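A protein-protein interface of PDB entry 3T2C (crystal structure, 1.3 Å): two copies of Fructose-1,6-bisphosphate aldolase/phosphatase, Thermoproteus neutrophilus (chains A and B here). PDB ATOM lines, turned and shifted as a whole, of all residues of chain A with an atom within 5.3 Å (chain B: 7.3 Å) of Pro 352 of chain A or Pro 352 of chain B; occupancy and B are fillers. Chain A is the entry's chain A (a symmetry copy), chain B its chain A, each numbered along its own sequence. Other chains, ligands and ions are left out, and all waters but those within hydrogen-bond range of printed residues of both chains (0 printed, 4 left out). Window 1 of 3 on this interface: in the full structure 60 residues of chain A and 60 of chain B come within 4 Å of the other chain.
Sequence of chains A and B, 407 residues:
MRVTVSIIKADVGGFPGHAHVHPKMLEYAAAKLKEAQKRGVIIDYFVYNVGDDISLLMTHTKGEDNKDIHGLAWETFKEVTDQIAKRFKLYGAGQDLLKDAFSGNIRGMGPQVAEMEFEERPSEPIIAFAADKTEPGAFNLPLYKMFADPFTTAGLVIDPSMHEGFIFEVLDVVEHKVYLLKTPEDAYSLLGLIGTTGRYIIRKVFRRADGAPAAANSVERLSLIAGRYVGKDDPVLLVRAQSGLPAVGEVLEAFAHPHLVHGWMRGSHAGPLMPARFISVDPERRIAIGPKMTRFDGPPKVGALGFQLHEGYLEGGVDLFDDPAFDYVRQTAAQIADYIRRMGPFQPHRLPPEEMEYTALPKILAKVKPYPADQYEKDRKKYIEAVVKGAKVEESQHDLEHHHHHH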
ATOM      1  N   HIS A 262      23.233  -9.518 -26.034  1.00  0.00           N
ATOM      2  CA  HIS A 262      22.029 -10.315 -26.182  1.00  0.00           C
ATOM      3  C   HIS A 262      20.915  -9.560 -26.849  1.00  0.00           C
ATOM      4  O   HIS A 262      20.653  -8.406 -26.439  1.00  0.00           O
ATOM      5  CB  HIS A 262      21.565 -10.753 -24.812  1.00  0.00           C
ATOM      6  CG  HIS A 262      22.480 -11.660 -24.088  1.00  0.00           C
ATOM      7  ND1 HIS A 262      23.585 -12.346 -24.479  1.00  0.00           N
ATOM      8  CD2 HIS A 262      22.193 -12.149 -22.864  1.00  0.00           C
ATOM      9  CE1 HIS A 262      24.045 -13.068 -23.434  1.00  0.00           C
ATOM     10  NE2 HIS A 262      23.135 -13.035 -22.531  1.00  0.00           N
ATOM     11  N   GLN A 347      23.230 -22.434 -28.683  1.00  0.00           N
ATOM     12  CA  GLN A 347      23.960 -21.629 -27.706  1.00  0.00           C
ATOM     13  C   GLN A 347      25.457 -21.753 -28.030  1.00  0.00           C
ATOM     14  O   GLN A 347      25.926 -22.833 -28.403  1.00  0.00           O
ATOM     15  CB  GLN A 347      23.816 -22.149 -26.266  1.00  0.00           C
ATOM     16  CG  GLN A 347      22.457 -21.823 -25.642  1.00  0.00           C
ATOM     17  CD  GLN A 347      22.427 -22.248 -24.195  1.00  0.00           C
ATOM     18  OE1 GLN A 347      21.768 -23.200 -23.896  1.00  0.00           O
ATOM     19  NE2 GLN A 347      23.064 -21.488 -23.243  1.00  0.00           N
ATOM     20  N   ARG A 350      22.461 -18.662 -29.960  1.00  0.00           N
ATOM     21  CA  ARG A 350      21.145 -18.630 -29.384  1.00  0.00           C
ATOM     22  C   ARG A 350      21.305 -18.406 -27.891  1.00  0.00           C
ATOM     23  O   ARG A 350      22.239 -18.895 -27.271  1.00  0.00           O
ATOM     24  CB  ARG A 350      20.394 -19.937 -29.640  1.00  0.00           C
ATOM     25  CG  ARG A 350      18.893 -19.831 -29.507  1.00  0.00           C
ATOM     26  CD  ARG A 350      18.275 -21.096 -28.969  1.00  0.00           C
ATOM     27  NE  ARG A 350      18.622 -21.240 -27.569  1.00  0.00           N
ATOM     28  CZ  ARG A 350      18.487 -22.351 -26.862  1.00  0.00           C
ATOM     29  NH1 ARG A 350      18.764 -22.318 -25.581  1.00  0.00           N
ATOM     30  NH2 ARG A 350      18.063 -23.461 -27.416  1.00  0.00           N
ATOM     31  N   LEU A 351      20.348 -17.707 -27.271  1.00  0.00           N
ATOM     32  CA  LEU A 351      20.427 -17.381 -25.891  1.00  0.00           C
ATOM     33  C   LEU A 351      20.103 -18.550 -24.982  1.00  0.00           C
ATOM     34  O   LEU A 351      19.508 -19.554 -25.366  1.00  0.00           O
ATOM     35  CB  LEU A 351      19.504 -16.202 -25.544  1.00  0.00           C
ATOM     36  CG  LEU A 351      19.983 -14.841 -26.100  1.00  0.00           C
ATOM     37  CD1 LEU A 351      19.026 -13.729 -25.717  1.00  0.00           C
ATOM     38  CD2 LEU A 351      21.442 -14.540 -25.860  1.00  0.00           C
ATOM     39  N   PRO A 352      20.481 -18.457 -23.710  1.00  0.00           N
ATOM     40  CA  PRO A 352      20.186 -19.478 -22.727  1.00  0.00           C
ATOM     41  C   PRO A 352      18.670 -19.668 -22.575  1.00  0.00           C
ATOM     42  O   PRO A 352      17.919 -18.757 -22.821  1.00  0.00           O
ATOM     43  CB  PRO A 352      20.883 -18.971 -21.447  1.00  0.00           C
ATOM     44  CG  PRO A 352      21.875 -18.027 -21.900  1.00  0.00           C
ATOM     45  CD  PRO A 352      21.272 -17.378 -23.088  1.00  0.00           C
ATOM     46  N   PRO A 353      18.371 -20.856 -21.881  1.00  0.00           N
ATOM     47  CA  PRO A 353      17.031 -21.365 -21.695  1.00  0.00           C
ATOM     48  C   PRO A 353      16.214 -20.417 -20.831  1.00  0.00           C
ATOM     49  O   PRO A 353      15.010 -20.286 -21.116  1.00  0.00           O
ATOM     50  CB  PRO A 353      17.212 -22.750 -21.047  1.00  0.00           C
ATOM     51  CG  PRO A 353      18.534 -22.940 -20.721  1.00  0.00           C
ATOM     52  CD  PRO A 353      19.354 -21.897 -21.492  1.00  0.00           C
ATOM     53  N   GLU A 354      16.775 -19.672 -19.912  1.00  0.00           N
ATOM     54  CA  GLU A 354      16.003 -18.693 -19.094  1.00  0.00           C
ATOM     55  C   GLU A 354      15.474 -17.518 -19.938  1.00  0.00           C
ATOM     56  O   GLU A 354      14.513 -16.872 -19.625  1.00  0.00           O
ATOM     57  CB  GLU A 354      16.864 -18.062 -17.959  1.00  0.00           C
ATOM     58  CG  GLU A 354      17.852 -18.933 -17.063  1.00  0.00           C
ATOM     59  CD  GLU A 354      18.621 -18.163 -15.886  1.00  0.00           C
ATOM     60  OE1 GLU A 354      18.543 -16.939 -15.833  1.00  0.00           O
ATOM     61  OE2 GLU A 354      19.292 -18.842 -15.019  1.00  0.00           O
ATOM     62  N   GLU A 355      16.143 -17.112 -20.966  1.00  0.00           N
ATOM     63  CA  GLU A 355      15.525 -16.166 -21.816  1.00  0.00           C
ATOM     64  C   GLU A 355      14.589 -16.815 -22.826  1.00  0.00           C
ATOM     65  O   GLU A 355      13.614 -16.197 -23.167  1.00  0.00           O
ATOM     66  CB  GLU A 355      16.668 -15.372 -22.532  1.00  0.00           C
ATOM     67  CG  GLU A 355      16.246 -14.196 -23.486  1.00  0.00           C
ATOM     68  CD  GLU A 355      16.354 -12.616 -23.437  1.00  0.00           C
ATOM     69  OE1 GLU A 355      15.674 -12.041 -24.515  1.00  0.00           O
ATOM     70  OE2 GLU A 355      17.083 -11.998 -22.527  1.00  0.00           O
ATOM     71  N   MET A 356      14.890 -18.082 -23.267  1.00  0.00           N
ATOM     72  CA  MET A 356      14.024 -18.749 -24.142  1.00  0.00           C
ATOM     73  C   MET A 356      12.659 -19.063 -23.504  1.00  0.00           C
ATOM     74  O   MET A 356      11.700 -19.237 -24.237  1.00  0.00           O
ATOM     75  CB  MET A 356      14.690 -19.996 -24.740  1.00  0.00           C
ATOM     76  CG  MET A 356      15.953 -19.771 -25.776  1.00  0.00           C
ATOM     77  SD  MET A 356      15.886 -18.479 -26.726  1.00  0.00           S
ATOM     78  CE  MET A 356      14.638 -19.389 -27.890  1.00  0.00           C
ATOM     79  N   GLY B 195      19.899 -27.173 -29.165  1.00  0.00           N
ATOM     80  CA  GLY B 195      20.517 -25.861 -29.034  1.00  0.00           C
ATOM     81  C   GLY B 195      20.843 -25.447 -27.630  1.00  0.00           C
ATOM     82  O   GLY B 195      21.697 -24.586 -27.420  1.00  0.00           O
ATOM     83  N   THR B 196      20.163 -26.056 -26.650  1.00  0.00           N
ATOM     84  CA  THR B 196      20.466 -25.912 -25.231  1.00  0.00           C
ATOM     85  C   THR B 196      21.546 -26.945 -24.886  1.00  0.00           C
ATOM     86  O   THR B 196      21.223 -28.019 -24.361  1.00  0.00           O
ATOM     87  CB  THR B 196      19.214 -26.026 -24.404  1.00  0.00           C
ATOM     88  OG1 THR B 196      18.252 -25.061 -24.877  1.00  0.00           O
ATOM     89  CG2 THR B 196      19.487 -25.803 -22.909  1.00  0.00           C
ATOM     90  N   HIS B 262      30.955 -24.076 -25.019  1.00  0.00           N
ATOM     91  CA  HIS B 262      31.085 -23.762 -23.608  1.00  0.00           C
ATOM     92  C   HIS B 262      32.205 -24.513 -22.948  1.00  0.00           C
ATOM     93  O   HIS B 262      32.291 -25.747 -23.153  1.00  0.00           O
ATOM     94  CB  HIS B 262      29.789 -24.112 -22.912  1.00  0.00           C
ATOM     95  CG  HIS B 262      28.610 -23.324 -23.324  1.00  0.00           C
ATOM     96  ND1 HIS B 262      28.478 -22.201 -24.077  1.00  0.00           N
ATOM     97  CD2 HIS B 262      27.390 -23.511 -22.779  1.00  0.00           C
ATOM     98  CE1 HIS B 262      27.172 -21.859 -24.129  1.00  0.00           C
ATOM     99  NE2 HIS B 262      26.567 -22.572 -23.250  1.00  0.00           N
ATOM    100  N   SER B 268      33.880 -21.878 -17.489  1.00  0.00           N
ATOM    101  CA  SER B 268      33.024 -20.733 -17.311  1.00  0.00           C
ATOM    102  C   SER B 268      32.933 -19.768 -18.459  1.00  0.00           C
ATOM    103  O   SER B 268      32.409 -18.680 -18.320  1.00  0.00           O
ATOM    104  CB  SER B 268      33.443 -19.977 -16.035  1.00  0.00           C
ATOM    105  OG  SER B 268      33.319 -20.769 -14.870  1.00  0.00           O
ATOM    106  N   GLN B 347      28.880 -12.092 -19.928  1.00  0.00           N
ATOM    107  CA  GLN B 347      28.105 -12.917 -20.853  1.00  0.00           C
ATOM    108  C   GLN B 347      28.020 -12.161 -22.187  1.00  0.00           C
ATOM    109  O   GLN B 347      27.878 -10.933 -22.199  1.00  0.00           O
ATOM    110  CB  GLN B 347      26.646 -13.116 -20.409  1.00  0.00           C
ATOM    111  CG  GLN B 347      26.498 -14.119 -19.262  1.00  0.00           C
ATOM    112  CD  GLN B 347      25.040 -14.361 -18.961  1.00  0.00           C
ATOM    113  OE1 GLN B 347      24.585 -13.909 -17.951  1.00  0.00           O
ATOM    114  NE2 GLN B 347      24.293 -15.170 -19.785  1.00  0.00           N
ATOM    115  N   PRO B 348      28.045 -12.867 -23.322  1.00  0.00           N
ATOM    116  CA  PRO B 348      28.042 -14.348 -23.470  1.00  0.00           C
ATOM    117  C   PRO B 348      29.445 -14.951 -23.529  1.00  0.00           C
ATOM    118  O   PRO B 348      29.508 -16.189 -23.697  1.00  0.00           O
ATOM    119  CB  PRO B 348      27.282 -14.558 -24.776  1.00  0.00           C
ATOM    120  CG  PRO B 348      27.667 -13.338 -25.564  1.00  0.00           C
ATOM    121  CD  PRO B 348      27.680 -12.225 -24.588  1.00  0.00           C
ATOM    122  N   HIS B 349      30.529 -14.219 -23.382  1.00  0.00           N
ATOM    123  CA  HIS B 349      31.819 -14.853 -23.248  1.00  0.00           C
ATOM    124  C   HIS B 349      31.919 -15.626 -21.945  1.00  0.00           C
ATOM    125  O   HIS B 349      32.371 -16.768 -21.951  1.00  0.00           O
ATOM    126  CB  HIS B 349      32.936 -13.865 -23.393  1.00  0.00           C
ATOM    127  CG  HIS B 349      34.318 -14.480 -23.214  1.00  0.00           C
ATOM    128  ND1 HIS B 349      34.717 -15.660 -23.838  1.00  0.00           N
ATOM    129  CD2 HIS B 349      35.398 -14.052 -22.537  1.00  0.00           C
ATOM    130  CE1 HIS B 349      36.003 -15.866 -23.485  1.00  0.00           C
ATOM    131  NE2 HIS B 349      36.438 -14.913 -22.696  1.00  0.00           N
ATOM    132  N   ARG B 350      31.525 -15.023 -20.856  1.00  0.00           N
ATOM    133  CA  ARG B 350      31.309 -15.742 -19.631  1.00  0.00           C
ATOM    134  C   ARG B 350      29.992 -16.485 -19.765  1.00  0.00           C
ATOM    135  O   ARG B 350      29.047 -16.001 -20.372  1.00  0.00           O
ATOM    136  CB  ARG B 350      31.257 -14.796 -18.432  1.00  0.00           C
ATOM    137  CG  ARG B 350      31.511 -15.460 -17.099  1.00  0.00           C
ATOM    138  CD  ARG B 350      30.721 -14.827 -15.983  1.00  0.00           C
ATOM    139  NE  ARG B 350      29.319 -15.156 -16.143  1.00  0.00           N
ATOM    140  CZ  ARG B 350      28.319 -14.554 -15.517  1.00  0.00           C
ATOM    141  NH1 ARG B 350      27.102 -15.008 -15.695  1.00  0.00           N
ATOM    142  NH2 ARG B 350      28.533 -13.538 -14.717  1.00  0.00           N
ATOM    143  N   LEU B 351      29.885 -17.661 -19.135  1.00  0.00           N
ATOM    144  CA  LEU B 351      28.726 -18.472 -19.245  1.00  0.00           C
ATOM    145  C   LEU B 351      27.564 -17.969 -18.410  1.00  0.00           C
ATOM    146  O   LEU B 351      27.699 -17.171 -17.485  1.00  0.00           O
ATOM    147  CB  LEU B 351      29.027 -19.929 -18.862  1.00  0.00           C
ATOM    148  CG  LEU B 351      29.897 -20.685 -19.893  1.00  0.00           C
ATOM    149  CD1 LEU B 351      30.152 -22.112 -19.448  1.00  0.00           C
ATOM    150  CD2 LEU B 351      29.456 -20.530 -21.327  1.00  0.00           C
ATOM    151  N   PRO B 352      26.354 -18.435 -18.703  1.00  0.00           N
ATOM    152  CA  PRO B 352      25.171 -18.077 -17.950  1.00  0.00           C
ATOM    153  C   PRO B 352      25.308 -18.506 -16.482  1.00  0.00           C
ATOM    154  O   PRO B 352      26.018 -19.435 -16.187  1.00  0.00           O
ATOM    155  CB  PRO B 352      24.025 -18.785 -18.702  1.00  0.00           C
ATOM    156  CG  PRO B 352      24.541 -19.052 -20.022  1.00  0.00           C
ATOM    157  CD  PRO B 352      25.984 -19.325 -19.821  1.00  0.00           C
ATOM    158  N   PRO B 353      24.331 -17.890 -15.677  1.00  0.00           N
ATOM    159  CA  PRO B 353      24.287 -18.002 -14.236  1.00  0.00           C
ATOM    160  C   PRO B 353      24.014 -19.439 -13.819  1.00  0.00           C
ATOM    161  O   PRO B 353      24.590 -19.851 -12.797  1.00  0.00           O
ATOM    162  CB  PRO B 353      23.176 -17.034 -13.790  1.00  0.00           C
ATOM    163  CG  PRO B 353      22.514 -16.547 -14.893  1.00  0.00           C
ATOM    164  CD  PRO B 353      23.394 -16.828 -16.119  1.00  0.00           C
ATOM    165  N   GLU B 354      23.310 -20.248 -14.570  1.00  0.00           N
ATOM    166  CA  GLU B 354      23.080 -21.676 -14.210  1.00  0.00           C
ATOM    167  C   GLU B 354      24.376 -22.508 -14.267  1.00  0.00           C
ATOM    168  O   GLU B 354      24.531 -23.515 -13.634  1.00  0.00           O
ATOM    169  CB  GLU B 354      22.072 -22.373 -15.173  1.00  0.00           C
ATOM    170  CG  GLU B 354      20.730 -21.660 -15.654  1.00  0.00           C
ATOM    171  CD  GLU B 354      19.753 -22.524 -16.587  1.00  0.00           C
ATOM    172  OE1 GLU B 354      20.149 -23.606 -17.012  1.00  0.00           O
ATOM    173  OE2 GLU B 354      18.577 -22.072 -16.860  1.00  0.00           O
ATOM    174  N   GLU B 355      25.301 -22.198 -15.113  1.00  0.00           N
ATOM    175  CA  GLU B 355      26.543 -22.865 -14.996  1.00  0.00           C
ATOM    176  C   GLU B 355      27.447 -22.229 -13.949  1.00  0.00           C
ATOM    177  O   GLU B 355      28.193 -22.950 -13.337  1.00  0.00           O
ATOM    178  CB  GLU B 355      27.213 -22.845 -16.411  1.00  0.00           C
ATOM    179  CG  GLU B 355      28.585 -23.595 -16.572  1.00  0.00           C
ATOM    180  CD  GLU B 355      29.065 -24.912 -17.312  1.00  0.00           C
ATOM    181  OE1 GLU B 355      30.399 -25.193 -17.003  1.00  0.00           O
ATOM    182  OE2 GLU B 355      28.287 -25.552 -18.165  1.00  0.00           O
ATOM    183  N   MET B 356      27.341 -20.876 -13.737  1.00  0.00           N
ATOM    184  CA  MET B 356      28.101 -20.256 -12.737  1.00  0.00           C
ATOM    185  C   MET B 356      27.718 -20.726 -11.322  1.00  0.00           C
ATOM    186  O   MET B 356      28.541 -20.613 -10.429  1.00  0.00           O
ATOM    187  CB  MET B 356      28.062 -18.728 -12.876  1.00  0.00           C
ATOM    188  CG  MET B 356      28.798 -18.055 -14.189  1.00  0.00           C
ATOM    189  SD  MET B 356      30.127 -18.782 -14.721  1.00  0.00           S
ATOM    190  CE  MET B 356      31.151 -17.972 -13.295  1.00  0.00           C
ATOM    191  N   GLU B 357      26.516 -21.275 -11.146  1.00  0.00           N
ATOM    192  CA  GLU B 357      26.090 -21.773  -9.818  1.00  0.00           C
ATOM    193  C   GLU B 357      27.005 -22.916  -9.339  1.00  0.00           C
ATOM    194  O   GLU B 357      27.093 -23.157  -8.156  1.00  0.00           O
ATOM    195  CB  GLU B 357      24.644 -22.255  -9.931  1.00  0.00           C
ATOM    196  CG  GLU B 357      24.022 -22.512  -8.593  1.00  0.00           C
ATOM    197  CD  GLU B 357      23.422 -21.287  -7.832  1.00  0.00           C
ATOM    198  OE1 GLU B 357      23.888 -20.911  -6.737  1.00  0.00           O
ATOM    199  OE2 GLU B 357      22.400 -20.756  -8.299  1.00  0.00           O
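The backbone NH of Gln 347 of chain A is in hydrogen-bond range of the backbone carbonyl oxygen of Gly 195 of chain B, 2.9 Å away. The guanidinium group of Arg 350 of chain A lies within hydrogen-bond range of the side-chain hydroxyl of Thr 196 of chain B, 2.9 Å away.
His 262 of chain A touches Gln 347 of chain B (NE2 to NE2, 3.7 Å). CB of Pro 348 of chain B touches CE1 of His 262 of chain A, at 3.8 Å. Gln 347 of chain A touches Thr 196 of chain B. Gln 347 of chain A touches His 262 of chain B (NE2 to NE2, 3.7 Å). Arg 350 of chain A touches Gly 195 of chain B (NH2 to C, 3.4 Å). Pro 352 of chain A touches Pro 352 of chain B. Thr 196 of chain B touches Pro 353 of chain A. OE2 of Glu 354 of chain B touches CG of Pro 353 of chain A, at 3.96 Å. Glu 354 of chain A touches Pro 353 of chain B. OE2 of Glu 354 of chain A touches CG of Glu 354 of chain B, 3.2 Å away.
Printed residues of chain B within 4 Å of Gln 347 of chain A: Gly 195, Thr 196 and His 262. Printed residues of chain B within 4 Å of Arg 350 of chain A: Gly 195 and Thr 196. Pro 352 of chain A touches just one residue of chain B: Pro 352 (3.4 Å). Of the printed residues of chain B, Pro 353 of chain A touches Thr 196 and Glu 354. Of the printed residues of chain B, Glu 354 of chain A touches Pro 353 and Glu 354. Of the printed residues of chain A, Pro 348 of chain B touches His 262. Pro 352 of chain B touches just one residue of chain A: Pro 352 (3.4 Å). Glu 355 of chain B touches none of the printed residues of chain A. The nearest printed residue of chain A that does not touch Gln 347 of chain B is Pro 352 of chain A (4.3 Å).
Printed residues of chain A that touch a printed residue of chain B: His 262, Gln 347, Arg 350, Pro 352, Pro 353 and Glu 354. Of the 15 printed residues of chain B, 8 touch a printed residue of chain A.
His 262 of chain A touches Gln 347 of chain B, and with the chains exchanged Gln 347 of chain A touches His 262 of chain B. Pro 352 of chain A touches its own counterpart, Pro 352 of chain B. Pro 353 of chain A touches Glu 354 of chain B, and with the chains exchanged Glu 354 of chain A touches Pro 353 of chain B. Glu 354 of chain A touches its own counterpart, Glu 354 of chain B.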
